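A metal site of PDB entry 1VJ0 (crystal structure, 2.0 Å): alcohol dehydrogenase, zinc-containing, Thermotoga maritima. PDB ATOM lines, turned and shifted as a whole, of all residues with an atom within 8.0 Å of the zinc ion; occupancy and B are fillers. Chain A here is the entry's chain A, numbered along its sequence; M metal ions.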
ATOM      1  N   ILE A 110      19.589  22.485 -17.481  1.00  0.00           N
ATOM      2  CA  ILE A 110      19.079  21.113 -17.434  1.00  0.00           C
ATOM      3  C   ILE A 110      17.828  21.124 -18.298  1.00  0.00           C
ATOM      4  O   ILE A 110      17.011  22.027 -18.206  1.00  0.00           O
ATOM      5  CB  ILE A 110      18.694  20.732 -16.007  1.00  0.00           C
ATOM      6  CG1 ILE A 110      19.952  20.629 -15.102  1.00  0.00           C
ATOM      7  CG2 ILE A 110      17.866  19.411 -15.989  1.00  0.00           C
ATOM      8  CD1 ILE A 110      19.586  20.286 -13.674  1.00  0.00           C
ATOM      9  N   THR A 111      17.767  20.168 -19.202  1.00  0.00           N
ATOM     10  CA  THR A 111      16.639  20.042 -20.130  1.00  0.00           C
ATOM     11  C   THR A 111      15.821  18.841 -19.685  1.00  0.00           C
ATOM     12  O   THR A 111      16.274  18.060 -18.876  1.00  0.00           O
ATOM     13  CB  THR A 111      17.156  19.909 -21.608  1.00  0.00           C
ATOM     14  OG1 THR A 111      17.951  18.726 -21.798  1.00  0.00           O
ATOM     15  CG2 THR A 111      18.092  21.071 -21.942  1.00  0.00           C
ATOM     16  N   CYS A 112      14.633  18.705 -20.224  1.00  0.00           N
ATOM     17  CA  CYS A 112      13.677  17.705 -19.766  1.00  0.00           C
ATOM     18  C   CYS A 112      14.001  16.281 -20.189  1.00  0.00           C
ATOM     19  O   CYS A 112      13.669  15.345 -19.461  1.00  0.00           O
ATOM     20  CB  CYS A 112      12.259  18.095 -20.131  1.00  0.00           C
ATOM     21  SG  CYS A 112      11.743  17.885 -21.867  1.00  0.00           S
ATOM     22  N   GLY A 113      14.673  16.110 -21.326  1.00  0.00           N
ATOM     23  CA  GLY A 113      14.945  14.791 -21.823  1.00  0.00           C
ATOM     24  C   GLY A 113      13.741  14.013 -22.324  1.00  0.00           C
ATOM     25  O   GLY A 113      13.877  12.804 -22.530  1.00  0.00           O
ATOM     26  N   GLU A 114      12.629  14.700 -22.608  1.00  0.00           N
ATOM     27  CA  GLU A 114      11.346  14.086 -22.966  1.00  0.00           C
ATOM     28  C   GLU A 114      10.631  14.753 -24.159  1.00  0.00           C
ATOM     29  O   GLU A 114       9.736  14.163 -24.747  1.00  0.00           O
ATOM     30  CB  GLU A 114      10.425  14.065 -21.751  1.00  0.00           C
ATOM     31  CG  GLU A 114      11.053  13.258 -20.620  1.00  0.00           C
ATOM     32  CD  GLU A 114      10.066  12.942 -19.547  1.00  0.00           C
ATOM     33  OE1 GLU A 114       9.358  13.890 -19.121  1.00  0.00           O
ATOM     34  OE2 GLU A 114      10.006  11.744 -19.137  1.00  0.00           O
ATOM     35  N   CYS A 115      11.025  15.962 -24.540  1.00  0.00           N
ATOM     36  CA  CYS A 115      10.261  16.686 -25.525  1.00  0.00           C
ATOM     37  C   CYS A 115      10.796  16.439 -26.940  1.00  0.00           C
ATOM     38  O   CYS A 115      11.808  15.755 -27.146  1.00  0.00           O
ATOM     39  CB  CYS A 115      10.263  18.167 -25.205  1.00  0.00           C
ATOM     40  SG  CYS A 115      11.849  18.917 -25.476  1.00  0.00           S
ATOM     41  N   TYR A 116      10.099  17.025 -27.898  1.00  0.00           N
ATOM     42  CA  TYR A 116      10.483  16.972 -29.299  1.00  0.00           C
ATOM     43  C   TYR A 116      11.932  17.391 -29.502  1.00  0.00           C
ATOM     44  O   TYR A 116      12.671  16.769 -30.252  1.00  0.00           O
ATOM     45  CB  TYR A 116       9.594  17.883 -30.138  1.00  0.00           C
ATOM     46  CG  TYR A 116       9.954  17.971 -31.614  1.00  0.00           C
ATOM     47  CD1 TYR A 116       9.492  17.023 -32.543  1.00  0.00           C
ATOM     48  CD2 TYR A 116      10.793  18.962 -32.073  1.00  0.00           C
ATOM     49  CE1 TYR A 116       9.827  17.102 -33.870  1.00  0.00           C
ATOM     50  CE2 TYR A 116      11.139  19.036 -33.393  1.00  0.00           C
ATOM     51  CZ  TYR A 116      10.661  18.128 -34.295  1.00  0.00           C
ATOM     52  OH  TYR A 116      10.999  18.278 -35.639  1.00  0.00           O
ATOM     53  N   TRP A 117      12.330  18.481 -28.846  1.00  0.00           N
ATOM     54  CA  TRP A 117      13.660  18.998 -29.074  1.00  0.00           C
ATOM     55  C   TRP A 117      14.732  18.140 -28.430  1.00  0.00           C
ATOM     56  O   TRP A 117      15.801  17.924 -29.052  1.00  0.00           O
ATOM     57  CB  TRP A 117      13.791  20.454 -28.661  1.00  0.00           C
ATOM     58  CG  TRP A 117      13.035  21.395 -29.547  1.00  0.00           C
ATOM     59  CD1 TRP A 117      13.461  21.955 -30.722  1.00  0.00           C
ATOM     60  CD2 TRP A 117      11.699  21.874 -29.355  1.00  0.00           C
ATOM     61  NE1 TRP A 117      12.478  22.769 -31.242  1.00  0.00           N
ATOM     62  CE2 TRP A 117      11.407  22.754 -30.415  1.00  0.00           C
ATOM     63  CE3 TRP A 117      10.726  21.674 -28.349  1.00  0.00           C
ATOM     64  CZ2 TRP A 117      10.169  23.398 -30.549  1.00  0.00           C
ATOM     65  CZ3 TRP A 117       9.487  22.321 -28.492  1.00  0.00           C
ATOM     66  CH2 TRP A 117       9.244  23.187 -29.553  1.00  0.00           C
ATOM     67  N   CYS A 118      14.500  17.688 -27.196  1.00  0.00           N
ATOM     68  CA  CYS A 118      15.431  16.827 -26.516  1.00  0.00           C
ATOM     69  C   CYS A 118      15.513  15.439 -27.197  1.00  0.00           C
ATOM     70  O   CYS A 118      16.571  14.870 -27.261  1.00  0.00           O
ATOM     71  CB  CYS A 118      15.025  16.626 -25.085  1.00  0.00           C
ATOM     72  SG  CYS A 118      15.162  18.115 -24.008  1.00  0.00           S
ATOM     73  N   LYS A 119      14.407  14.908 -27.707  1.00  0.00           N
ATOM     74  CA  LYS A 119      14.386  13.492 -28.140  1.00  0.00           C
ATOM     75  C   LYS A 119      14.264  13.240 -29.639  1.00  0.00           C
ATOM     76  O   LYS A 119      14.635  12.171 -30.090  1.00  0.00           O
ATOM     77  CB  LYS A 119      13.294  12.705 -27.407  1.00  0.00           C
ATOM     78  CG  LYS A 119      13.671  12.340 -25.957  1.00  0.00           C
ATOM     79  CD  LYS A 119      14.657  11.129 -25.998  1.00  0.00           C
ATOM     80  CE  LYS A 119      15.042  10.602 -24.629  1.00  0.00           C
ATOM     81  NZ  LYS A 119      13.873  10.263 -23.757  1.00  0.00           N
ATOM     82  N   GLU A 123      18.067  18.837 -30.382  1.00  0.00           N
ATOM     83  CA  GLU A 123      18.441  20.218 -30.132  1.00  0.00           C
ATOM     84  C   GLU A 123      18.038  20.620 -28.709  1.00  0.00           C
ATOM     85  O   GLU A 123      17.174  21.461 -28.517  1.00  0.00           O
ATOM     86  CB  GLU A 123      17.706  21.124 -31.130  1.00  0.00           C
ATOM     87  CG  GLU A 123      18.038  20.855 -32.593  1.00  0.00           C
ATOM     88  CD  GLU A 123      17.003  21.369 -33.589  1.00  0.00           C
ATOM     89  OE1 GLU A 123      15.774  21.360 -33.340  1.00  0.00           O
ATOM     90  OE2 GLU A 123      17.435  21.747 -34.681  1.00  0.00           O
ATOM     91  N   PRO A 124      18.693  20.041 -27.701  1.00  0.00           N
ATOM     92  CA  PRO A 124      18.297  20.278 -26.317  1.00  0.00           C
ATOM     93  C   PRO A 124      18.405  21.720 -25.842  1.00  0.00           C
ATOM     94  O   PRO A 124      17.675  22.099 -24.923  1.00  0.00           O
ATOM     95  CB  PRO A 124      19.259  19.386 -25.502  1.00  0.00           C
ATOM     96  CG  PRO A 124      20.171  18.747 -26.461  1.00  0.00           C
ATOM     97  CD  PRO A 124      19.843  19.142 -27.809  1.00  0.00           C
ATOM     98  N   TYR A 125      19.257  22.515 -26.480  1.00  0.00           N
ATOM     99  CA  TYR A 125      19.353  23.961 -26.173  1.00  0.00           C
ATOM    100  C   TYR A 125      18.005  24.618 -26.450  1.00  0.00           C
ATOM    101  O   TYR A 125      17.700  25.718 -25.921  1.00  0.00           O
ATOM    102  CB  TYR A 125      20.532  24.629 -26.960  1.00  0.00           C
ATOM    103  CG  TYR A 125      20.690  24.154 -28.369  1.00  0.00           C
ATOM    104  CD1 TYR A 125      21.448  23.015 -28.688  1.00  0.00           C
ATOM    105  CD2 TYR A 125      20.019  24.778 -29.402  1.00  0.00           C
ATOM    106  CE1 TYR A 125      21.504  22.545 -29.987  1.00  0.00           C
ATOM    107  CE2 TYR A 125      20.082  24.340 -30.701  1.00  0.00           C
ATOM    108  CZ  TYR A 125      20.796  23.201 -30.983  1.00  0.00           C
ATOM    109  OH  TYR A 125      20.793  22.810 -32.300  1.00  0.00           O
ATOM    110  N   LEU A 126      17.166  23.995 -27.292  1.00  0.00           N
ATOM    111  CA  LEU A 126      15.822  24.547 -27.586  1.00  0.00           C
ATOM    112  C   LEU A 126      14.648  24.003 -26.712  1.00  0.00           C
ATOM    113  O   LEU A 126      13.488  24.332 -26.926  1.00  0.00           O
ATOM    114  CB  LEU A 126      15.454  24.397 -29.072  1.00  0.00           C
ATOM    115  CG  LEU A 126      16.451  24.959 -30.068  1.00  0.00           C
ATOM    116  CD1 LEU A 126      16.078  24.710 -31.515  1.00  0.00           C
ATOM    117  CD2 LEU A 126      16.665  26.403 -29.797  1.00  0.00           C
ATOM    118  N   CYS A 127      14.972  23.218 -25.707  1.00  0.00           N
ATOM    119  CA  CYS A 127      13.967  22.605 -24.846  1.00  0.00           C
ATOM    120  C   CYS A 127      13.163  23.747 -24.189  1.00  0.00           C
ATOM    121  O   CYS A 127      13.732  24.678 -23.643  1.00  0.00           O
ATOM    122  CB  CYS A 127      14.667  21.783 -23.803  1.00  0.00           C
ATOM    123  SG  CYS A 127      13.570  21.151 -22.500  1.00  0.00           S
ATOM    124  N   PRO A 128      11.842  23.738 -24.292  1.00  0.00           N
ATOM    125  CA  PRO A 128      11.054  24.782 -23.651  1.00  0.00           C
ATOM    126  C   PRO A 128      11.030  24.679 -22.102  1.00  0.00           C
ATOM    127  O   PRO A 128      10.475  25.556 -21.463  1.00  0.00           O
ATOM    128  CB  PRO A 128       9.652  24.572 -24.234  1.00  0.00           C
ATOM    129  CG  PRO A 128       9.611  23.086 -24.637  1.00  0.00           C
ATOM    130  CD  PRO A 128      11.029  22.725 -24.968  1.00  0.00           C
ATOM    131  N   ASN A 129      11.568  23.609 -21.525  1.00  0.00           N
ATOM    132  CA  ASN A 129      11.446  23.365 -20.090  1.00  0.00           C
ATOM    133  C   ASN A 129      12.817  23.496 -19.468  1.00  0.00           C
ATOM    134  O   ASN A 129      13.070  22.920 -18.433  1.00  0.00           O
ATOM    135  CB  ASN A 129      10.929  21.936 -19.860  1.00  0.00           C
ATOM    136  CG  ASN A 129       9.563  21.671 -20.510  1.00  0.00           C
ATOM    137  OD1 ASN A 129       8.613  22.378 -20.228  1.00  0.00           O
ATOM    138  ND2 ASN A 129       9.461  20.618 -21.348  1.00  0.00           N
ATOM    139  N   ARG A 130      13.701  24.221 -20.124  1.00  0.00           N
ATOM    140  CA  ARG A 130      15.128  24.326 -19.710  1.00  0.00           C
ATOM    141  C   ARG A 130      15.273  25.161 -18.410  1.00  0.00           C
ATOM    142  O   ARG A 130      14.734  26.260 -18.303  1.00  0.00           O
ATOM    143  CB  ARG A 130      15.913  24.970 -20.865  1.00  0.00           C
ATOM    144  CG  ARG A 130      17.394  24.996 -20.764  1.00  0.00           C
ATOM    145  CD  ARG A 130      18.111  25.410 -22.091  1.00  0.00           C
ATOM    146  NE  ARG A 130      19.465  25.732 -21.772  1.00  0.00           N
ATOM    147  CZ  ARG A 130      19.898  26.945 -21.396  1.00  0.00           C
ATOM    148  NH1 ARG A 130      19.073  28.003 -21.366  1.00  0.00           N
ATOM    149  NH2 ARG A 130      21.160  27.081 -21.058  1.00  0.00           N
HETATM  150 ZN    ZN M   1      13.085  19.023 -23.477  1.00  0.00          ZN
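SG of Cys 127 lies close to N of Asn 129 (3.3 Å). OG1 of Thr 111 lies close to SG of Cys 118 (3.6 Å). The side-chain sulfur (SG) of Cys 115 sits close to the backbone NH (N) of Trp 117, at 3.4 Å. The backbone NH (N) of Glu 114 lies close to the side-chain sulfur (SG) of Cys 112, 3.4 Å away. NZ of Lys 119 sits at hydrogen-bond distance from O of Gly 113 (2.8 Å). The backbone NH of Gly 113 sits close to the side-chain sulfur of Cys 118 (3.4 Å). ND2 of Asn 129 sits close to SG of Cys 112, at 3.6 Å.
N of Gly 113 touches the zinc ion, at 3.95 Å. Of the 18 residues printed, 5 come within 4 Å of the zinc ion. The nearest printed residue that does not touch the zinc ion is Glu 114 (4.4 Å).
The zinc ion is bound by SG of Cys 118 (2.3 Å), SG of Cys 115 (2.4 Å), SG of Cys 112 (2.4 Å) and SG of Cys 127 (2.4 Å). The zinc ion has four donor atoms within binding distance.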
